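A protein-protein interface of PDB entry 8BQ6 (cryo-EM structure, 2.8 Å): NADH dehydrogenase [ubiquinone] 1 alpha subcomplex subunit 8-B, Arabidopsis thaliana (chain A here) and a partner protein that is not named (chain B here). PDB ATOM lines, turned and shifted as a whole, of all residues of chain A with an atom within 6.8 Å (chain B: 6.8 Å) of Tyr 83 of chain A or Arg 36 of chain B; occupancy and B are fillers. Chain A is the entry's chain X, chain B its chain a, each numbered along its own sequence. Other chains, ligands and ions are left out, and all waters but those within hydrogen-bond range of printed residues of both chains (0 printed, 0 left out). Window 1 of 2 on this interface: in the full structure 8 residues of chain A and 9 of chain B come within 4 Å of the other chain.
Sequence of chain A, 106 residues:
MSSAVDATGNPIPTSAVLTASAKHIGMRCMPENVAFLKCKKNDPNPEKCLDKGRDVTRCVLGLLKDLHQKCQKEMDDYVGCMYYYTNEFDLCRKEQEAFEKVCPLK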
ATOM      1  N   THR A  14       4.206 -20.299  29.942  1.00  0.00           N
ATOM      2  CA  THR A  14       4.976 -19.075  30.059  1.00  0.00           C
ATOM      3  C   THR A  14       4.719 -18.184  28.845  1.00  0.00           C
ATOM      4  O   THR A  14       4.035 -18.566  27.892  1.00  0.00           O
ATOM      5  CB  THR A  14       6.457 -19.409  30.211  1.00  0.00           C
ATOM      6  OG1 THR A  14       6.869 -20.243  29.121  1.00  0.00           O
ATOM      7  CG2 THR A  14       6.693 -20.143  31.515  1.00  0.00           C
ATOM      8  N   SER A  15       5.264 -16.964  28.888  1.00  0.00           N
ATOM      9  CA  SER A  15       5.062 -16.039  27.777  1.00  0.00           C
ATOM     10  C   SER A  15       5.709 -16.569  26.507  1.00  0.00           C
ATOM     11  O   SER A  15       5.210 -16.328  25.402  1.00  0.00           O
ATOM     12  CB  SER A  15       5.615 -14.655  28.122  1.00  0.00           C
ATOM     13  OG  SER A  15       7.027 -14.672  28.226  1.00  0.00           O
ATOM     14  N   ALA A  16       6.818 -17.297  26.645  1.00  0.00           N
ATOM     15  CA  ALA A  16       7.460 -17.898  25.483  1.00  0.00           C
ATOM     16  C   ALA A  16       6.555 -18.939  24.832  1.00  0.00           C
ATOM     17  O   ALA A  16       6.338 -18.908  23.616  1.00  0.00           O
ATOM     18  CB  ALA A  16       8.803 -18.509  25.884  1.00  0.00           C
ATOM     19  N   VAL A  17       5.995 -19.856  25.630  1.00  0.00           N
ATOM     20  CA  VAL A  17       5.114 -20.886  25.075  1.00  0.00           C
ATOM     21  C   VAL A  17       3.869 -20.262  24.459  1.00  0.00           C
ATOM     22  O   VAL A  17       3.490 -20.586  23.325  1.00  0.00           O
ATOM     23  CB  VAL A  17       4.739 -21.929  26.144  1.00  0.00           C
ATOM     24  CG1 VAL A  17       3.981 -23.065  25.493  1.00  0.00           C
ATOM     25  CG2 VAL A  17       5.985 -22.480  26.809  1.00  0.00           C
ATOM     26  N   TYR A  78      11.526 -24.106  19.153  1.00  0.00           N
ATOM     27  CA  TYR A  78      10.917 -22.806  18.908  1.00  0.00           C
ATOM     28  C   TYR A  78      10.712 -22.038  20.206  1.00  0.00           C
ATOM     29  O   TYR A  78      11.039 -20.850  20.289  1.00  0.00           O
ATOM     30  CB  TYR A  78       9.593 -22.980  18.170  1.00  0.00           C
ATOM     31  CG  TYR A  78       9.039 -21.691  17.624  1.00  0.00           C
ATOM     32  CD1 TYR A  78       9.874 -20.618  17.352  1.00  0.00           C
ATOM     33  CD2 TYR A  78       7.685 -21.548  17.371  1.00  0.00           C
ATOM     34  CE1 TYR A  78       9.375 -19.440  16.852  1.00  0.00           C
ATOM     35  CE2 TYR A  78       7.177 -20.372  16.869  1.00  0.00           C
ATOM     36  CZ  TYR A  78       8.027 -19.321  16.611  1.00  0.00           C
ATOM     37  OH  TYR A  78       7.529 -18.144  16.109  1.00  0.00           O
ATOM     38  N   VAL A  79      10.178 -22.704  21.231  1.00  0.00           N
ATOM     39  CA  VAL A  79       9.942 -22.058  22.517  1.00  0.00           C
ATOM     40  C   VAL A  79      11.258 -21.612  23.139  1.00  0.00           C
ATOM     41  O   VAL A  79      11.347 -20.529  23.728  1.00  0.00           O
ATOM     42  CB  VAL A  79       9.161 -23.010  23.443  1.00  0.00           C
ATOM     43  CG1 VAL A  79       9.182 -22.520  24.879  1.00  0.00           C
ATOM     44  CG2 VAL A  79       7.737 -23.177  22.945  1.00  0.00           C
ATOM     45  N   GLY A  80      12.302 -22.435  23.016  1.00  0.00           N
ATOM     46  CA  GLY A  80      13.599 -22.048  23.546  1.00  0.00           C
ATOM     47  C   GLY A  80      14.157 -20.817  22.862  1.00  0.00           C
ATOM     48  O   GLY A  80      14.675 -19.905  23.514  1.00  0.00           O
ATOM     49  N   CYS A  81      14.041 -20.766  21.534  1.00  0.00           N
ATOM     50  CA  CYS A  81      14.490 -19.582  20.810  1.00  0.00           C
ATOM     51  C   CYS A  81      13.681 -18.355  21.210  1.00  0.00           C
ATOM     52  O   CYS A  81      14.241 -17.272  21.422  1.00  0.00           O
ATOM     53  CB  CYS A  81      14.392 -19.823  19.306  1.00  0.00           C
ATOM     54  SG  CYS A  81      15.414 -18.723  18.317  1.00  0.00           S
ATOM     55  N   MET A  82      12.364 -18.516  21.336  1.00  0.00           N
ATOM     56  CA  MET A  82      11.499 -17.378  21.619  1.00  0.00           C
ATOM     57  C   MET A  82      11.742 -16.848  23.022  1.00  0.00           C
ATOM     58  O   MET A  82      11.652 -15.639  23.263  1.00  0.00           O
ATOM     59  CB  MET A  82      10.039 -17.779  21.440  1.00  0.00           C
ATOM     60  CG  MET A  82       9.582 -17.682  20.002  1.00  0.00           C
ATOM     61  SD  MET A  82       9.477 -16.000  19.376  1.00  0.00           S
ATOM     62  CE  MET A  82       7.817 -15.582  19.865  1.00  0.00           C
ATOM     63  N   TYR A  83      12.036 -17.741  23.966  1.00  0.00           N
ATOM     64  CA  TYR A  83      12.429 -17.283  25.288  1.00  0.00           C
ATOM     65  C   TYR A  83      13.765 -16.557  25.236  1.00  0.00           C
ATOM     66  O   TYR A  83      13.920 -15.490  25.841  1.00  0.00           O
ATOM     67  CB  TYR A  83      12.499 -18.453  26.265  1.00  0.00           C
ATOM     68  CG  TYR A  83      13.232 -18.070  27.519  1.00  0.00           C
ATOM     69  CD1 TYR A  83      12.592 -17.359  28.519  1.00  0.00           C
ATOM     70  CD2 TYR A  83      14.569 -18.391  27.692  1.00  0.00           C
ATOM     71  CE1 TYR A  83      13.258 -16.985  29.658  1.00  0.00           C
ATOM     72  CE2 TYR A  83      15.243 -18.021  28.826  1.00  0.00           C
ATOM     73  CZ  TYR A  83      14.582 -17.320  29.808  1.00  0.00           C
ATOM     74  OH  TYR A  83      15.254 -16.952  30.948  1.00  0.00           O
ATOM     75  N   TYR A  84      14.738 -17.114  24.512  1.00  0.00           N
ATOM     76  CA  TYR A  84      16.053 -16.491  24.460  1.00  0.00           C
ATOM     77  C   TYR A  84      15.968 -15.077  23.895  1.00  0.00           C
ATOM     78  O   TYR A  84      16.582 -14.147  24.434  1.00  0.00           O
ATOM     79  CB  TYR A  84      16.995 -17.360  23.632  1.00  0.00           C
ATOM     80  CG  TYR A  84      18.402 -16.840  23.531  1.00  0.00           C
ATOM     81  CD1 TYR A  84      19.306 -17.038  24.565  1.00  0.00           C
ATOM     82  CD2 TYR A  84      18.837 -16.180  22.394  1.00  0.00           C
ATOM     83  CE1 TYR A  84      20.595 -16.574  24.475  1.00  0.00           C
ATOM     84  CE2 TYR A  84      20.123 -15.714  22.294  1.00  0.00           C
ATOM     85  CZ  TYR A  84      21.000 -15.917  23.336  1.00  0.00           C
ATOM     86  OH  TYR A  84      22.288 -15.450  23.242  1.00  0.00           O
ATOM     87  N   TYR A  85      15.179 -14.886  22.839  1.00  0.00           N
ATOM     88  CA  TYR A  85      15.075 -13.606  22.152  1.00  0.00           C
ATOM     89  C   TYR A  85      13.879 -12.774  22.609  1.00  0.00           C
ATOM     90  O   TYR A  85      13.522 -11.803  21.934  1.00  0.00           O
ATOM     91  CB  TYR A  85      15.008 -13.822  20.643  1.00  0.00           C
ATOM     92  CG  TYR A  85      16.317 -14.230  20.023  1.00  0.00           C
ATOM     93  CD1 TYR A  85      17.445 -13.437  20.160  1.00  0.00           C
ATOM     94  CD2 TYR A  85      16.421 -15.393  19.279  1.00  0.00           C
ATOM     95  CE1 TYR A  85      18.642 -13.799  19.587  1.00  0.00           C
ATOM     96  CE2 TYR A  85      17.614 -15.764  18.700  1.00  0.00           C
ATOM     97  CZ  TYR A  85      18.722 -14.962  18.857  1.00  0.00           C
ATOM     98  OH  TYR A  85      19.916 -15.325  18.281  1.00  0.00           O
ATOM     99  N   THR A  86      13.251 -13.144  23.728  1.00  0.00           N
ATOM    100  CA  THR A  86      12.130 -12.407  24.328  1.00  0.00           C
ATOM    101  C   THR A  86      10.976 -12.209  23.340  1.00  0.00           C
ATOM    102  O   THR A  86      10.393 -11.128  23.224  1.00  0.00           O
ATOM    103  CB  THR A  86      12.596 -11.070  24.915  1.00  0.00           C
ATOM    104  OG1 THR A  86      13.865 -11.246  25.555  1.00  0.00           O
ATOM    105  CG2 THR A  86      11.602 -10.564  25.955  1.00  0.00           C
ATOM    106  N   ASN A  87      10.640 -13.286  22.631  1.00  0.00           N
ATOM    107  CA  ASN A  87       9.453 -13.357  21.776  1.00  0.00           C
ATOM    108  C   ASN A  87       9.540 -12.438  20.561  1.00  0.00           C
ATOM    109  O   ASN A  87       8.536 -11.866  20.131  1.00  0.00           O
ATOM    110  CB  ASN A  87       8.167 -13.073  22.561  1.00  0.00           C
ATOM    111  CG  ASN A  87       8.088 -13.857  23.852  1.00  0.00           C
ATOM    112  OD1 ASN A  87       7.481 -13.412  24.822  1.00  0.00           O
ATOM    113  ND2 ASN A  87       8.700 -15.033  23.872  1.00  0.00           N
ATOM    114  N   CYS A  92      13.607 -15.799  14.997  1.00  0.00           N
ATOM    115  CA  CYS A  92      13.273 -17.231  15.232  1.00  0.00           C
ATOM    116  C   CYS A  92      12.599 -17.828  13.994  1.00  0.00           C
ATOM    117  O   CYS A  92      11.728 -18.692  14.176  1.00  0.00           O
ATOM    118  CB  CYS A  92      12.322 -17.348  16.417  1.00  0.00           C
ATOM    119  SG  CYS A  92      12.836 -16.432  17.893  1.00  0.00           S
ATOM    120  N   TYR B  27      27.312  -5.914  26.145  1.00  0.00           N
ATOM    121  CA  TYR B  27      26.349  -6.921  25.708  1.00  0.00           C
ATOM    122  C   TYR B  27      26.520  -8.242  26.457  1.00  0.00           C
ATOM    123  O   TYR B  27      25.528  -8.899  26.798  1.00  0.00           O
ATOM    124  CB  TYR B  27      26.485  -7.139  24.208  1.00  0.00           C
ATOM    125  CG  TYR B  27      25.583  -8.203  23.649  1.00  0.00           C
ATOM    126  CD1 TYR B  27      26.038  -9.503  23.493  1.00  0.00           C
ATOM    127  CD2 TYR B  27      24.288  -7.909  23.250  1.00  0.00           C
ATOM    128  CE1 TYR B  27      25.230 -10.477  22.973  1.00  0.00           C
ATOM    129  CE2 TYR B  27      23.470  -8.881  22.722  1.00  0.00           C
ATOM    130  CZ  TYR B  27      23.948 -10.162  22.588  1.00  0.00           C
ATOM    131  OH  TYR B  27      23.143 -11.142  22.063  1.00  0.00           O
ATOM    132  N   HIS B  30      25.397  -7.998  30.411  1.00  0.00           N
ATOM    133  CA  HIS B  30      23.950  -8.032  30.592  1.00  0.00           C
ATOM    134  C   HIS B  30      23.410  -9.440  30.383  1.00  0.00           C
ATOM    135  O   HIS B  30      22.553  -9.910  31.142  1.00  0.00           O
ATOM    136  CB  HIS B  30      23.288  -7.039  29.632  1.00  0.00           C
ATOM    137  CG  HIS B  30      21.835  -6.799  29.901  1.00  0.00           C
ATOM    138  ND1 HIS B  30      20.840  -7.596  29.380  1.00  0.00           N
ATOM    139  CD2 HIS B  30      21.210  -5.857  30.647  1.00  0.00           C
ATOM    140  CE1 HIS B  30      19.664  -7.151  29.785  1.00  0.00           C
ATOM    141  NE2 HIS B  30      19.862  -6.097  30.557  1.00  0.00           N
ATOM    142  N   LYS B  31      23.928 -10.137  29.373  1.00  0.00           N
ATOM    143  CA  LYS B  31      23.479 -11.494  29.090  1.00  0.00           C
ATOM    144  C   LYS B  31      23.822 -12.450  30.226  1.00  0.00           C
ATOM    145  O   LYS B  31      23.031 -13.339  30.556  1.00  0.00           O
ATOM    146  CB  LYS B  31      24.100 -11.979  27.787  1.00  0.00           C
ATOM    147  CG  LYS B  31      23.338 -13.091  27.138  1.00  0.00           C
ATOM    148  CD  LYS B  31      24.084 -13.594  25.932  1.00  0.00           C
ATOM    149  CE  LYS B  31      24.299 -15.082  26.034  1.00  0.00           C
ATOM    150  NZ  LYS B  31      25.121 -15.577  24.907  1.00  0.00           N
ATOM    151  N   ALA B  32      25.010 -12.304  30.818  1.00  0.00           N
ATOM    152  CA  ALA B  32      25.383 -13.167  31.935  1.00  0.00           C
ATOM    153  C   ALA B  32      24.494 -12.915  33.145  1.00  0.00           C
ATOM    154  O   ALA B  32      24.104 -13.854  33.849  1.00  0.00           O
ATOM    155  CB  ALA B  32      26.854 -12.958  32.293  1.00  0.00           C
ATOM    156  N   TYR B  33      24.159 -11.652  33.397  1.00  0.00           N
ATOM    157  CA  TYR B  33      23.354 -11.315  34.562  1.00  0.00           C
ATOM    158  C   TYR B  33      21.901 -11.738  34.400  1.00  0.00           C
ATOM    159  O   TYR B  33      21.265 -12.155  35.372  1.00  0.00           O
ATOM    160  CB  TYR B  33      23.433  -9.818  34.835  1.00  0.00           C
ATOM    161  CG  TYR B  33      22.704  -9.419  36.090  1.00  0.00           C
ATOM    162  CD1 TYR B  33      23.346  -9.430  37.317  1.00  0.00           C
ATOM    163  CD2 TYR B  33      21.370  -9.045  36.050  1.00  0.00           C
ATOM    164  CE1 TYR B  33      22.680  -9.070  38.469  1.00  0.00           C
ATOM    165  CE2 TYR B  33      20.695  -8.689  37.193  1.00  0.00           C
ATOM    166  CZ  TYR B  33      21.353  -8.700  38.399  1.00  0.00           C
ATOM    167  OH  TYR B  33      20.675  -8.337  39.536  1.00  0.00           O
ATOM    168  N   HIS B  34      21.349 -11.619  33.195  1.00  0.00           N
ATOM    169  CA  HIS B  34      19.944 -11.928  32.981  1.00  0.00           C
ATOM    170  C   HIS B  34      19.718 -13.284  32.324  1.00  0.00           C
ATOM    171  O   HIS B  34      18.589 -13.783  32.349  1.00  0.00           O
ATOM    172  CB  HIS B  34      19.290 -10.823  32.144  1.00  0.00           C
ATOM    173  CG  HIS B  34      19.290  -9.485  32.817  1.00  0.00           C
ATOM    174  ND1 HIS B  34      20.337  -8.597  32.705  1.00  0.00           N
ATOM    175  CD2 HIS B  34      18.372  -8.886  33.612  1.00  0.00           C
ATOM    176  CE1 HIS B  34      20.063  -7.506  33.399  1.00  0.00           C
ATOM    177  NE2 HIS B  34      18.878  -7.657  33.959  1.00  0.00           N
ATOM    178  N   GLY B  35      20.756 -13.902  31.766  1.00  0.00           N
ATOM    179  CA  GLY B  35      20.643 -15.214  31.171  1.00  0.00           C
ATOM    180  C   GLY B  35      20.193 -15.226  29.727  1.00  0.00           C
ATOM    181  O   GLY B  35      20.099 -16.306  29.132  1.00  0.00           O
ATOM    182  N   ARG B  36      19.902 -14.069  29.153  1.00  0.00           N
ATOM    183  CA  ARG B  36      19.530 -13.926  27.755  1.00  0.00           C
ATOM    184  C   ARG B  36      19.889 -12.515  27.319  1.00  0.00           C
ATOM    185  O   ARG B  36      20.027 -11.620  28.158  1.00  0.00           O
ATOM    186  CB  ARG B  36      18.035 -14.197  27.532  1.00  0.00           C
ATOM    187  CG  ARG B  36      17.108 -13.523  28.509  1.00  0.00           C
ATOM    188  CD  ARG B  36      15.685 -13.926  28.192  1.00  0.00           C
ATOM    189  NE  ARG B  36      14.703 -13.319  29.080  1.00  0.00           N
ATOM    190  CZ  ARG B  36      13.394 -13.418  28.909  1.00  0.00           C
ATOM    191  NH1 ARG B  36      12.880 -14.070  27.878  1.00  0.00           N
ATOM    192  NH2 ARG B  36      12.578 -12.855  29.794  1.00  0.00           N
ATOM    193  N   PRO B  37      20.065 -12.288  26.019  1.00  0.00           N
ATOM    194  CA  PRO B  37      20.480 -10.961  25.560  1.00  0.00           C
ATOM    195  C   PRO B  37      19.398  -9.922  25.793  1.00  0.00           C
ATOM    196  O   PRO B  37      18.209 -10.228  25.905  1.00  0.00           O
ATOM    197  CB  PRO B  37      20.739 -11.169  24.067  1.00  0.00           C
ATOM    198  CG  PRO B  37      19.847 -12.282  23.697  1.00  0.00           C
ATOM    199  CD  PRO B  37      19.800 -13.193  24.886  1.00  0.00           C
ATOM    200  N   LYS B  38      19.836  -8.670  25.880  1.00  0.00           N
ATOM    201  CA  LYS B  38      18.897  -7.586  26.112  1.00  0.00           C
ATOM    202  C   LYS B  38      17.978  -7.429  24.909  1.00  0.00           C
ATOM    203  O   LYS B  38      18.416  -7.474  23.757  1.00  0.00           O
ATOM    204  CB  LYS B  38      19.644  -6.284  26.399  1.00  0.00           C
ATOM    205  CG  LYS B  38      18.774  -5.048  26.323  1.00  0.00           C
ATOM    206  CD  LYS B  38      19.602  -3.823  26.047  1.00  0.00           C
ATOM    207  CE  LYS B  38      20.013  -3.181  27.352  1.00  0.00           C
ATOM    208  NZ  LYS B  38      18.894  -2.389  27.933  1.00  0.00           N
ATOM    209  N   HIS B  39      16.692  -7.266  25.187  1.00  0.00           N
ATOM    210  CA  HIS B  39      15.664  -7.193  24.162  1.00  0.00           C
ATOM    211  C   HIS B  39      15.369  -5.733  23.841  1.00  0.00           C
ATOM    212  O   HIS B  39      15.015  -4.955  24.733  1.00  0.00           O
ATOM    213  CB  HIS B  39      14.403  -7.912  24.632  1.00  0.00           C
ATOM    214  CG  HIS B  39      13.213  -7.671  23.766  1.00  0.00           C
ATOM    215  ND1 HIS B  39      11.970  -7.370  24.277  1.00  0.00           N
ATOM    216  CD2 HIS B  39      13.078  -7.677  22.422  1.00  0.00           C
ATOM    217  CE1 HIS B  39      11.116  -7.209  23.284  1.00  0.00           C
ATOM    218  NE2 HIS B  39      11.763  -7.389  22.148  1.00  0.00           N
ATOM    219  N   HIS B  42      11.599  -3.137  24.833  1.00  0.00           N
ATOM    220  CA  HIS B  42      10.864  -3.658  25.976  1.00  0.00           C
ATOM    221  C   HIS B  42       9.759  -2.686  26.355  1.00  0.00           C
ATOM    222  O   HIS B  42      10.026  -1.588  26.850  1.00  0.00           O
ATOM    223  CB  HIS B  42      11.812  -3.881  27.147  1.00  0.00           C
ATOM    224  CG  HIS B  42      11.526  -5.131  27.910  1.00  0.00           C
ATOM    225  ND1 HIS B  42      11.614  -6.383  27.342  1.00  0.00           N
ATOM    226  CD2 HIS B  42      11.137  -5.324  29.192  1.00  0.00           C
ATOM    227  CE1 HIS B  42      11.302  -7.295  28.244  1.00  0.00           C
ATOM    228  NE2 HIS B  42      11.006  -6.678  29.374  1.00  0.00           N
ATOM    229  N   ASP B  46       5.791  -6.491  27.561  1.00  0.00           N
ATOM    230  CA  ASP B  46       6.903  -7.373  27.909  1.00  0.00           C
ATOM    231  C   ASP B  46       7.200  -7.327  29.398  1.00  0.00           C
ATOM    232  O   ASP B  46       7.533  -8.351  30.008  1.00  0.00           O
ATOM    233  CB  ASP B  46       8.140  -6.986  27.109  1.00  0.00           C
ATOM    234  CG  ASP B  46       7.910  -7.070  25.629  1.00  0.00           C
ATOM    235  OD1 ASP B  46       8.150  -6.068  24.928  1.00  0.00           O
ATOM    236  OD2 ASP B  46       7.478  -8.142  25.166  1.00  0.00           O
ATOM    237  N   GLU B  50       6.951 -10.528  31.877  1.00  0.00           N
ATOM    238  CA  GLU B  50       8.005 -10.961  32.785  1.00  0.00           C
ATOM    239  C   GLU B  50       7.484 -11.082  34.215  1.00  0.00           C
ATOM    240  O   GLU B  50       7.784 -12.059  34.917  1.00  0.00           O
ATOM    241  CB  GLU B  50       9.180  -9.992  32.707  1.00  0.00           C
ATOM    242  CG  GLU B  50      10.218 -10.204  33.778  1.00  0.00           C
ATOM    243  CD  GLU B  50      11.392  -9.261  33.636  1.00  0.00           C
ATOM    244  OE1 GLU B  50      12.217  -9.198  34.571  1.00  0.00           O
ATOM    245  OE2 GLU B  50      11.491  -8.585  32.590  1.00  0.00           O
ATOM    246  N   ASP B  53       5.322 -14.171  34.317  1.00  0.00           N
ATOM    247  CA  ASP B  53       6.150 -15.357  34.159  1.00  0.00           C
ATOM    248  C   ASP B  53       6.895 -15.692  35.435  1.00  0.00           C
ATOM    249  O   ASP B  53       7.160 -16.868  35.698  1.00  0.00           O
ATOM    250  CB  ASP B  53       7.148 -15.145  33.026  1.00  0.00           C
ATOM    251  CG  ASP B  53       6.676 -15.721  31.721  1.00  0.00           C
ATOM    252  OD1 ASP B  53       5.455 -15.909  31.556  1.00  0.00           O
ATOM    253  OD2 ASP B  53       7.531 -15.976  30.852  1.00  0.00           O
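The backbone NH of Ser 15 of chain A sits at hydrogen-bond distance from the side-chain carboxylate of Asp 53 of chain B. The backbone carbonyl oxygen of Tyr 83 of chain A is in hydrogen-bond range of the guanidinium group of Arg 36 of chain B (2.7 Å). The side-chain amino group of Lys 31 of chain B sits at hydrogen-bond distance from the side-chain hydroxyl of Tyr 84 of chain A (3.3 Å).
A ring nitrogen (ND1) of His 39 of chain B lies within hydrogen-bond range of a ring nitrogen (ND1) of His 42 of chain B, 3.2 Å away.
Of the printed residues of chain B, Thr 14 of chain A touches Asp 53 (3.5 Å). Of the printed residues of chain B, Ser 15 of chain A touches Asp 53 (2.9 Å). Of chain B, only Arg 36 (2.7 Å) comes within 4 Å of Tyr 83 of chain A. Printed residues of chain B within 4 Å of Tyr 84 of chain A: Lys 31 (3.3 Å), Arg 36 (3.4 Å) and Pro 37 (3.4 Å). Printed residues of chain B within 4 Å of Thr 86 of chain A: Arg 36 (3.8 Å) and His 39 (3.5 Å). Printed residues of chain A within 4 Å of Lys 31 of chain B: Tyr 84 (3.3 Å). Of chain A, only Tyr 83 (2.7 Å), Tyr 84 (3.4 Å) and Thr 86 (3.8 Å) come within 4 Å of Arg 36 of chain B. The nearest residue of chain A that does not touch Arg 36 of chain B is Met 82 of chain A (5.0 Å).
Among the printed residues, merely in contact across the chains: Tyr 84 of chain A with Pro 37 of chain B, Tyr 84 of chain A with Arg 36 of chain B, Thr 86 of chain A with His 39 of chain B, Thr 14 of chain A with Asp 53 of chain B and Thr 86 of chain A with Arg 36 of chain B.
Hydrophobic or aromatic side chains of chain A that line the printed part of chain B: Tyr 83 and Tyr 84.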
